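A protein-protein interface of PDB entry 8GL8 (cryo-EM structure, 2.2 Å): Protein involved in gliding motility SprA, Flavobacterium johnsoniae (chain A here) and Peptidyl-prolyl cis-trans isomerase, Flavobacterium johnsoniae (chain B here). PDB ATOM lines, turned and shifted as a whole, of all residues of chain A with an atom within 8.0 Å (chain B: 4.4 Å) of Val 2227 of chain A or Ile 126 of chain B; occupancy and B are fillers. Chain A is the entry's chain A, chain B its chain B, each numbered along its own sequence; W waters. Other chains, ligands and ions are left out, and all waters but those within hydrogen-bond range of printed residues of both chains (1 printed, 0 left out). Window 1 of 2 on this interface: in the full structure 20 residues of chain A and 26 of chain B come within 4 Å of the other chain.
N of Val 2227 of chain A lies within hydrogen-bond range of O of Thr 124 of chain B (2.6 Å). NZ of Lys 130 of chain B sits at hydrogen-bond distance from OE1 of Gln 2228 of chain A. N of Ile 126 of chain B is in hydrogen-bond range of O of Pro 2225 of chain A (3.2 Å). O of Thr 124 of chain B is in hydrogen-bond range of N of Gln 2228 of chain A. O of Ser 2224 of chain A sits at hydrogen-bond distance from OH of Tyr 152 of chain B (3.2 Å). The backbone carbonyl oxygen (O) of Ser 2223 of chain A lies within hydrogen-bond range of the side-chain hydroxyl (OH) of Tyr 152 of chain B, at 3.1 Å.
Of the 19 printed residues of chain A, 7 touch a printed residue of chain B. Printed residues of chain B that touch a printed residue of chain A: Thr 124, Leu 125, Ile 126, Trp 129, Lys 130 and Tyr 152. Among the printed residues, 16 pairs touch across the chains.
Among the printed residues, pairs that only touch across the chains: His 2105 of chain A with Tyr 152 of chain B, Pro 2225 of chain A with Thr 124 of chain B, Pro 2225 of chain A with Leu 125 of chain B, Pro 2225 of chain A with Trp 129 of chain B, Pro 2225 of chain A with Tyr 152 of chain B, Lys 2226 of chain A with Thr 124 of chain B, Lys 2226 of chain A with Leu 125 of chain B, Val 2227 of chain A with Leu 125 of chain B, Val 2227 of chain A with Ile 126 of chain B and Val 2227 of chain A with Tyr 152 of chain B.
Val 2227 of chain A touches just these residues of chain B: Thr 124 (2.6 Å), Leu 125 (3.8 Å), Ile 126 (3.7 Å) and Tyr 152 (3.8 Å). Ile 126 of chain B touches two residues of chain A. No residue of chain A comes within 4 Å of Pro 127 of chain B. Of the printed residues of chain B, Gln 2228 of chain A touches Thr 124 and Lys 130. Of the printed residues of chain A, Lys 130 of chain B touches Gln 2228. Printed residues of chain A within 4 Å of Thr 124 of chain B: Pro 2225, Lys 2226, Val 2227 and Gln 2228. Gly 151 of chain B touches none of the printed residues of chain A. Val 2230 of chain A touches none of the printed residues of chain B.
The backbone NH (N) of Lys 2226 of chain A lies close to the side-chain hydroxyl (OG) of Ser 2224 of chain A (3.4 Å). NE2 of Gln 2228 of chain A sits at hydrogen-bond distance from O of Thr 2232 of chain A, 2.8 Å away. NZ of Lys 2226 of chain A sits at hydrogen-bond distance from OH of Tyr 2235 of chain A (2.7 Å). The backbone NH (N) of Tyr 2235 of chain A lies within hydrogen-bond range of the backbone carbonyl oxygen (O) of Val 2227 of chain A. NZ of Lys 2226 of chain A is in hydrogen-bond range of O of Gln 2228 of chain A, at 3.0 Å. OG of Ser 2224 of chain A lies within hydrogen-bond range of OD1 of Asn 2222 of chain A (2.7 Å).
Water W1 bridges the side-chain hydroxyl of Tyr 152 of chain B (2.5 Å) and the backbone carbonyl oxygen of Ser 2223 of chain A (2.6 Å).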
ATOM      1  N   HIS A2105      28.588  21.650  28.609  1.00  0.00           N
ATOM      2  CA  HIS A2105      27.233  22.086  28.937  1.00  0.00           C
ATOM      3  C   HIS A2105      26.438  20.970  29.614  1.00  0.00           C
ATOM      4  O   HIS A2105      25.967  21.134  30.744  1.00  0.00           O
ATOM      5  CB  HIS A2105      26.520  22.576  27.672  1.00  0.00           C
ATOM      6  CG  HIS A2105      25.154  23.131  27.926  1.00  0.00           C
ATOM      7  ND1 HIS A2105      24.002  22.409  27.699  1.00  0.00           N
ATOM      8  CD2 HIS A2105      24.754  24.338  28.391  1.00  0.00           C
ATOM      9  CE1 HIS A2105      22.953  23.146  28.014  1.00  0.00           C
ATOM     10  NE2 HIS A2105      23.383  24.322  28.437  1.00  0.00           N
ATOM     11  N   GLY A2142      22.424  22.245  21.171  1.00  0.00           N
ATOM     12  CA  GLY A2142      22.699  23.665  21.154  1.00  0.00           C
ATOM     13  C   GLY A2142      23.930  24.096  20.396  1.00  0.00           C
ATOM     14  O   GLY A2142      24.249  25.287  20.384  1.00  0.00           O
ATOM     15  N   ASN A2147      27.241  27.545  14.801  1.00  0.00           N
ATOM     16  CA  ASN A2147      27.445  28.238  16.066  1.00  0.00           C
ATOM     17  C   ASN A2147      28.815  28.906  16.083  1.00  0.00           C
ATOM     18  O   ASN A2147      29.824  28.284  15.739  1.00  0.00           O
ATOM     19  CB  ASN A2147      27.313  27.262  17.233  1.00  0.00           C
ATOM     20  CG  ASN A2147      27.007  27.958  18.547  1.00  0.00           C
ATOM     21  OD1 ASN A2147      27.459  29.074  18.792  1.00  0.00           O
ATOM     22  ND2 ASN A2147      26.237  27.297  19.400  1.00  0.00           N
ATOM     23  N   ASP A2220      20.892  39.074  24.359  1.00  0.00           N
ATOM     24  CA  ASP A2220      20.163  37.811  24.325  1.00  0.00           C
ATOM     25  C   ASP A2220      20.726  36.797  25.310  1.00  0.00           C
ATOM     26  O   ASP A2220      20.030  35.840  25.662  1.00  0.00           O
ATOM     27  CB  ASP A2220      20.181  37.230  22.913  1.00  0.00           C
ATOM     28  CG  ASP A2220      19.367  38.049  21.935  1.00  0.00           C
ATOM     29  OD1 ASP A2220      18.415  38.727  22.372  1.00  0.00           O
ATOM     30  OD2 ASP A2220      19.679  38.018  20.726  1.00  0.00           O
ATOM     31  N   TYR A2221      21.966  36.983  25.754  1.00  0.00           N
ATOM     32  CA  TYR A2221      22.579  36.132  26.772  1.00  0.00           C
ATOM     33  C   TYR A2221      22.198  36.701  28.133  1.00  0.00           C
ATOM     34  O   TYR A2221      22.908  37.526  28.708  1.00  0.00           O
ATOM     35  CB  TYR A2221      24.088  36.071  26.578  1.00  0.00           C
ATOM     36  CG  TYR A2221      24.784  35.036  27.429  1.00  0.00           C
ATOM     37  CD1 TYR A2221      24.843  33.708  27.031  1.00  0.00           C
ATOM     38  CD2 TYR A2221      25.389  35.389  28.626  1.00  0.00           C
ATOM     39  CE1 TYR A2221      25.481  32.762  27.803  1.00  0.00           C
ATOM     40  CE2 TYR A2221      26.030  34.449  29.406  1.00  0.00           C
ATOM     41  CZ  TYR A2221      26.072  33.137  28.989  1.00  0.00           C
ATOM     42  OH  TYR A2221      26.708  32.196  29.762  1.00  0.00           O
ATOM     43  N   ASN A2222      21.059  36.253  28.655  1.00  0.00           N
ATOM     44  CA  ASN A2222      20.497  36.800  29.882  1.00  0.00           C
ATOM     45  C   ASN A2222      20.027  35.642  30.757  1.00  0.00           C
ATOM     46  O   ASN A2222      20.349  34.476  30.509  1.00  0.00           O
ATOM     47  CB  ASN A2222      19.369  37.791  29.564  1.00  0.00           C
ATOM     48  CG  ASN A2222      18.372  37.241  28.565  1.00  0.00           C
ATOM     49  OD1 ASN A2222      17.911  36.109  28.689  1.00  0.00           O
ATOM     50  ND2 ASN A2222      18.029  38.045  27.567  1.00  0.00           N
ATOM     51  N   SER A2223      19.260  35.970  31.793  1.00  0.00           N
ATOM     52  CA  SER A2223      18.774  34.991  32.756  1.00  0.00           C
ATOM     53  C   SER A2223      17.416  34.407  32.389  1.00  0.00           C
ATOM     54  O   SER A2223      16.874  33.611  33.161  1.00  0.00           O
ATOM     55  CB  SER A2223      18.698  35.621  34.149  1.00  0.00           C
ATOM     56  OG  SER A2223      17.904  36.795  34.132  1.00  0.00           O
ATOM     57  N   SER A2224      16.856  34.781  31.242  1.00  0.00           N
ATOM     58  CA  SER A2224      15.555  34.280  30.839  1.00  0.00           C
ATOM     59  C   SER A2224      15.640  32.804  30.458  1.00  0.00           C
ATOM     60  O   SER A2224      16.717  32.296  30.139  1.00  0.00           O
ATOM     61  CB  SER A2224      15.015  35.098  29.669  1.00  0.00           C
ATOM     62  OG  SER A2224      15.649  34.735  28.457  1.00  0.00           O
ATOM     63  N   PRO A2225      14.513  32.088  30.499  1.00  0.00           N
ATOM     64  CA  PRO A2225      14.524  30.681  30.064  1.00  0.00           C
ATOM     65  C   PRO A2225      14.844  30.497  28.590  1.00  0.00           C
ATOM     66  O   PRO A2225      15.190  29.381  28.186  1.00  0.00           O
ATOM     67  CB  PRO A2225      13.105  30.198  30.396  1.00  0.00           C
ATOM     68  CG  PRO A2225      12.287  31.440  30.503  1.00  0.00           C
ATOM     69  CD  PRO A2225      13.206  32.482  31.049  1.00  0.00           C
ATOM     70  N   LYS A2226      14.732  31.543  27.774  1.00  0.00           N
ATOM     71  CA  LYS A2226      15.060  31.439  26.358  1.00  0.00           C
ATOM     72  C   LYS A2226      16.570  31.329  26.185  1.00  0.00           C
ATOM     73  O   LYS A2226      17.311  32.251  26.538  1.00  0.00           O
ATOM     74  CB  LYS A2226      14.516  32.647  25.602  1.00  0.00           C
ATOM     75  CG  LYS A2226      14.766  32.610  24.105  1.00  0.00           C
ATOM     76  CD  LYS A2226      14.473  33.955  23.464  1.00  0.00           C
ATOM     77  CE  LYS A2226      13.961  33.791  22.042  1.00  0.00           C
ATOM     78  NZ  LYS A2226      14.976  33.179  21.141  1.00  0.00           N
ATOM     79  N   VAL A2227      17.027  30.204  25.640  1.00  0.00           N
ATOM     80  CA  VAL A2227      18.454  29.922  25.531  1.00  0.00           C
ATOM     81  C   VAL A2227      18.905  29.649  24.104  1.00  0.00           C
ATOM     82  O   VAL A2227      20.115  29.699  23.839  1.00  0.00           O
ATOM     83  CB  VAL A2227      18.867  28.747  26.446  1.00  0.00           C
ATOM     84  CG1 VAL A2227      18.805  29.167  27.903  1.00  0.00           C
ATOM     85  CG2 VAL A2227      17.979  27.538  26.195  1.00  0.00           C
ATOM     86  N   GLN A2228      17.996  29.365  23.177  1.00  0.00           N
ATOM     87  CA  GLN A2228      18.352  29.058  21.800  1.00  0.00           C
ATOM     88  C   GLN A2228      17.817  30.138  20.870  1.00  0.00           C
ATOM     89  O   GLN A2228      16.745  30.699  21.110  1.00  0.00           O
ATOM     90  CB  GLN A2228      17.816  27.689  21.381  1.00  0.00           C
ATOM     91  CG  GLN A2228      18.472  26.525  22.104  1.00  0.00           C
ATOM     92  CD  GLN A2228      17.860  25.191  21.736  1.00  0.00           C
ATOM     93  OE1 GLN A2228      16.884  24.754  22.344  1.00  0.00           O
ATOM     94  NE2 GLN A2228      18.432  24.532  20.737  1.00  0.00           N
ATOM     95  N   ASP A2229      18.573  30.430  19.816  1.00  0.00           N
ATOM     96  CA  ASP A2229      18.183  31.446  18.852  1.00  0.00           C
ATOM     97  C   ASP A2229      17.397  30.807  17.706  1.00  0.00           C
ATOM     98  O   ASP A2229      16.985  29.647  17.772  1.00  0.00           O
ATOM     99  CB  ASP A2229      19.411  32.211  18.354  1.00  0.00           C
ATOM    100  CG  ASP A2229      20.535  31.299  17.896  1.00  0.00           C
ATOM    101  OD1 ASP A2229      20.268  30.312  17.184  1.00  0.00           O
ATOM    102  OD2 ASP A2229      21.700  31.585  18.243  1.00  0.00           O
ATOM    103  N   VAL A2230      17.182  31.576  16.636  1.00  0.00           N
ATOM    104  CA  VAL A2230      16.415  31.098  15.492  1.00  0.00           C
ATOM    105  C   VAL A2230      17.112  29.946  14.777  1.00  0.00           C
ATOM    106  O   VAL A2230      16.463  29.190  14.046  1.00  0.00           O
ATOM    107  CB  VAL A2230      16.138  32.274  14.532  1.00  0.00           C
ATOM    108  CG1 VAL A2230      17.411  32.699  13.813  1.00  0.00           C
ATOM    109  CG2 VAL A2230      15.034  31.923  13.542  1.00  0.00           C
ATOM    110  N   THR A2232      18.588  27.492  16.442  1.00  0.00           N
ATOM    111  CA  THR A2232      18.652  26.465  17.483  1.00  0.00           C
ATOM    112  C   THR A2232      20.016  26.409  18.164  1.00  0.00           C
ATOM    113  O   THR A2232      20.340  25.421  18.828  1.00  0.00           O
ATOM    114  CB  THR A2232      18.275  25.076  16.946  1.00  0.00           C
ATOM    115  OG1 THR A2232      19.325  24.577  16.109  1.00  0.00           O
ATOM    116  CG2 THR A2232      16.979  25.137  16.149  1.00  0.00           C
ATOM    117  N   ASN A2233      20.821  27.455  18.018  1.00  0.00           N
ATOM    118  CA  ASN A2233      22.107  27.549  18.692  1.00  0.00           C
ATOM    119  C   ASN A2233      21.948  28.229  20.043  1.00  0.00           C
ATOM    120  O   ASN A2233      21.123  29.130  20.212  1.00  0.00           O
ATOM    121  CB  ASN A2233      23.112  28.329  17.843  1.00  0.00           C
ATOM    122  CG  ASN A2233      23.625  27.534  16.666  1.00  0.00           C
ATOM    123  OD1 ASN A2233      24.026  26.381  16.809  1.00  0.00           O
ATOM    124  ND2 ASN A2233      23.622  28.149  15.491  1.00  0.00           N
ATOM    125  N   PHE A2234      22.747  27.789  21.010  1.00  0.00           N
ATOM    126  CA  PHE A2234      22.797  28.471  22.294  1.00  0.00           C
ATOM    127  C   PHE A2234      23.353  29.878  22.121  1.00  0.00           C
ATOM    128  O   PHE A2234      24.247  30.114  21.304  1.00  0.00           O
ATOM    129  CB  PHE A2234      23.658  27.690  23.287  1.00  0.00           C
ATOM    130  CG  PHE A2234      22.977  26.488  23.868  1.00  0.00           C
ATOM    131  CD1 PHE A2234      21.647  26.547  24.250  1.00  0.00           C
ATOM    132  CD2 PHE A2234      23.666  25.302  24.041  1.00  0.00           C
ATOM    133  CE1 PHE A2234      21.019  25.443  24.786  1.00  0.00           C
ATOM    134  CE2 PHE A2234      23.043  24.195  24.576  1.00  0.00           C
ATOM    135  CZ  PHE A2234      21.718  24.266  24.949  1.00  0.00           C
ATOM    136  N   TYR A2235      22.807  30.817  22.886  1.00  0.00           N
ATOM    137  CA  TYR A2235      23.294  32.188  22.841  1.00  0.00           C
ATOM    138  C   TYR A2235      24.709  32.267  23.401  1.00  0.00           C
ATOM    139  O   TYR A2235      25.054  31.579  24.363  1.00  0.00           O
ATOM    140  CB  TYR A2235      22.366  33.112  23.627  1.00  0.00           C
ATOM    141  CG  TYR A2235      21.059  33.400  22.930  1.00  0.00           C
ATOM    142  CD1 TYR A2235      21.034  34.028  21.694  1.00  0.00           C
ATOM    143  CD2 TYR A2235      19.848  33.045  23.507  1.00  0.00           C
ATOM    144  CE1 TYR A2235      19.844  34.295  21.053  1.00  0.00           C
ATOM    145  CE2 TYR A2235      18.651  33.305  22.873  1.00  0.00           C
ATOM    146  CZ  TYR A2235      18.655  33.932  21.646  1.00  0.00           C
ATOM    147  OH  TYR A2235      17.466  34.198  21.008  1.00  0.00           O
ATOM    148  N   ASN A2236      25.527  33.113  22.787  1.00  0.00           N
ATOM    149  CA  ASN A2236      26.905  33.314  23.208  1.00  0.00           C
ATOM    150  C   ASN A2236      27.017  34.603  24.008  1.00  0.00           C
ATOM    151  O   ASN A2236      26.406  35.618  23.661  1.00  0.00           O
ATOM    152  CB  ASN A2236      27.841  33.358  21.999  1.00  0.00           C
ATOM    153  CG  ASN A2236      27.887  32.039  21.254  1.00  0.00           C
ATOM    154  OD1 ASN A2236      28.043  30.981  21.859  1.00  0.00           O
ATOM    155  ND2 ASN A2236      27.745  32.096  19.938  1.00  0.00           N
ATOM    156  N   THR B 124      12.779  27.499  21.998  1.00  0.00           N
ATOM    157  CA  THR B 124      13.974  28.239  22.362  1.00  0.00           C
ATOM    158  C   THR B 124      14.258  28.198  23.855  1.00  0.00           C
ATOM    159  O   THR B 124      15.255  28.776  24.300  1.00  0.00           O
ATOM    160  CB  THR B 124      13.839  29.692  21.901  1.00  0.00           C
ATOM    161  OG1 THR B 124      12.903  30.375  22.744  1.00  0.00           O
ATOM    162  CG2 THR B 124      13.339  29.745  20.467  1.00  0.00           C
ATOM    163  N   LEU B 125      13.416  27.532  24.634  1.00  0.00           N
ATOM    164  CA  LEU B 125      13.543  27.517  26.081  1.00  0.00           C
ATOM    165  C   LEU B 125      14.377  26.323  26.541  1.00  0.00           C
ATOM    166  O   LEU B 125      14.764  25.458  25.755  1.00  0.00           O
ATOM    167  CB  LEU B 125      12.161  27.497  26.733  1.00  0.00           C
ATOM    168  CG  LEU B 125      11.160  28.514  26.182  1.00  0.00           C
ATOM    169  CD1 LEU B 125       9.806  28.362  26.854  1.00  0.00           C
ATOM    170  CD2 LEU B 125      11.685  29.930  26.348  1.00  0.00           C
ATOM    171  N   ILE B 126      14.657  26.292  27.840  1.00  0.00           N
ATOM    172  CA  ILE B 126      15.453  25.229  28.447  1.00  0.00           C
ATOM    173  C   ILE B 126      14.670  23.924  28.376  1.00  0.00           C
ATOM    174  O   ILE B 126      13.433  23.951  28.302  1.00  0.00           O
ATOM    175  CB  ILE B 126      15.833  25.579  29.895  1.00  0.00           C
ATOM    176  CG1 ILE B 126      14.605  26.038  30.679  1.00  0.00           C
ATOM    177  CG2 ILE B 126      16.910  26.650  29.917  1.00  0.00           C
ATOM    178  CD1 ILE B 126      14.867  26.224  32.154  1.00  0.00           C
ATOM    179  N   PRO B 127      15.339  22.765  28.376  1.00  0.00           N
ATOM    180  CA  PRO B 127      14.605  21.494  28.258  1.00  0.00           C
ATOM    181  C   PRO B 127      13.577  21.273  29.353  1.00  0.00           C
ATOM    182  O   PRO B 127      12.536  20.653  29.094  1.00  0.00           O
ATOM    183  CB  PRO B 127      15.720  20.441  28.317  1.00  0.00           C
ATOM    184  CG  PRO B 127      16.940  21.158  27.867  1.00  0.00           C
ATOM    185  CD  PRO B 127      16.798  22.565  28.354  1.00  0.00           C
ATOM    186  N   GLY B 128      13.839  21.757  30.571  1.00  0.00           N
ATOM    187  CA  GLY B 128      12.864  21.608  31.638  1.00  0.00           C
ATOM    188  C   GLY B 128      11.527  22.228  31.286  1.00  0.00           C
ATOM    189  O   GLY B 128      10.474  21.613  31.469  1.00  0.00           O
ATOM    190  N   TRP B 129      11.552  23.451  30.755  1.00  0.00           N
ATOM    191  CA  TRP B 129      10.325  24.057  30.253  1.00  0.00           C
ATOM    192  C   TRP B 129       9.770  23.274  29.073  1.00  0.00           C
ATOM    193  O   TRP B 129       8.555  23.083  28.964  1.00  0.00           O
ATOM    194  CB  TRP B 129      10.575  25.510  29.856  1.00  0.00           C
ATOM    195  CG  TRP B 129      10.663  26.446  31.010  1.00  0.00           C
ATOM    196  CD1 TRP B 129      11.409  26.290  32.139  1.00  0.00           C
ATOM    197  CD2 TRP B 129       9.982  27.696  31.149  1.00  0.00           C
ATOM    198  NE1 TRP B 129      11.236  27.366  32.972  1.00  0.00           N
ATOM    199  CE2 TRP B 129      10.364  28.244  32.387  1.00  0.00           C
ATOM    200  CE3 TRP B 129       9.087  28.406  30.345  1.00  0.00           C
ATOM    201  CZ2 TRP B 129       9.881  29.467  32.841  1.00  0.00           C
ATOM    202  CZ3 TRP B 129       8.609  29.617  30.796  1.00  0.00           C
ATOM    203  CH2 TRP B 129       9.007  30.137  32.031  1.00  0.00           C
ATOM    204  N   LYS B 130      10.654  22.797  28.189  1.00  0.00           N
ATOM    205  CA  LYS B 130      10.214  22.069  27.003  1.00  0.00           C
ATOM    206  C   LYS B 130       9.396  20.838  27.362  1.00  0.00           C
ATOM    207  O   LYS B 130       8.501  20.449  26.605  1.00  0.00           O
ATOM    208  CB  LYS B 130      11.419  21.662  26.158  1.00  0.00           C
ATOM    209  CG  LYS B 130      11.867  22.700  25.153  1.00  0.00           C
ATOM    210  CD  LYS B 130      13.352  22.564  24.877  1.00  0.00           C
ATOM    211  CE  LYS B 130      13.735  23.247  23.582  1.00  0.00           C
ATOM    212  NZ  LYS B 130      14.701  22.431  22.796  1.00  0.00           N
ATOM    213  N   LEU B 150      18.958  19.832  32.706  1.00  0.00           N
ATOM    214  CA  LEU B 150      17.787  20.351  32.017  1.00  0.00           C
ATOM    215  C   LEU B 150      17.620  21.852  32.201  1.00  0.00           C
ATOM    216  O   LEU B 150      16.668  22.427  31.665  1.00  0.00           O
ATOM    217  CB  LEU B 150      16.524  19.628  32.495  1.00  0.00           C
ATOM    218  CG  LEU B 150      16.522  18.104  32.393  1.00  0.00           C
ATOM    219  CD1 LEU B 150      15.304  17.529  33.094  1.00  0.00           C
ATOM    220  CD2 LEU B 150      16.564  17.669  30.938  1.00  0.00           C
ATOM    221  N   GLY B 151      18.516  22.496  32.944  1.00  0.00           N
ATOM    222  CA  GLY B 151      18.447  23.927  33.158  1.00  0.00           C
ATOM    223  C   GLY B 151      19.482  24.687  32.358  1.00  0.00           C
ATOM    224  O   GLY B 151      19.374  24.794  31.133  1.00  0.00           O
ATOM    225  N   TYR B 152      20.498  25.220  33.037  1.00  0.00           N
ATOM    226  CA  TYR B 152      21.562  25.974  32.387  1.00  0.00           C
ATOM    227  C   TYR B 152      22.883  25.212  32.359  1.00  0.00           C
ATOM    228  O   TYR B 152      23.933  25.807  32.105  1.00  0.00           O
ATOM    229  CB  TYR B 152      21.734  27.334  33.063  1.00  0.00           C
ATOM    230  CG  TYR B 152      20.494  28.194  32.982  1.00  0.00           C
ATOM    231  CD1 TYR B 152      20.143  28.826  31.797  1.00  0.00           C
ATOM    232  CD2 TYR B 152      19.669  28.361  34.082  1.00  0.00           C
ATOM    233  CE1 TYR B 152      19.009  29.608  31.716  1.00  0.00           C
ATOM    234  CE2 TYR B 152      18.533  29.140  34.010  1.00  0.00           C
ATOM    235  CZ  TYR B 152      18.208  29.762  32.823  1.00  0.00           C
ATOM    236  OH  TYR B 152      17.076  30.538  32.749  1.00  0.00           O
ATOM    237  N   PHE B 168      10.694  26.800  39.230  1.00  0.00           N
ATOM    238  CA  PHE B 168       9.900  27.705  38.408  1.00  0.00           C
ATOM    239  C   PHE B 168       8.437  27.598  38.802  1.00  0.00           C
ATOM    240  O   PHE B 168       7.909  26.492  38.934  1.00  0.00           O
ATOM    241  CB  PHE B 168      10.060  27.386  36.918  1.00  0.00           C
ATOM    242  CG  PHE B 168      11.371  27.826  36.337  1.00  0.00           C
ATOM    243  CD1 PHE B 168      11.572  29.144  35.967  1.00  0.00           C
ATOM    244  CD2 PHE B 168      12.400  26.919  36.152  1.00  0.00           C
ATOM    245  CE1 PHE B 168      12.776  29.550  35.428  1.00  0.00           C
ATOM    246  CE2 PHE B 168      13.606  27.319  35.615  1.00  0.00           C
ATOM    247  CZ  PHE B 168      13.794  28.636  35.251  1.00  0.00           C
HETATM  248  O   HOH W   1      15.155  31.769  33.806  1.00  0.00           O
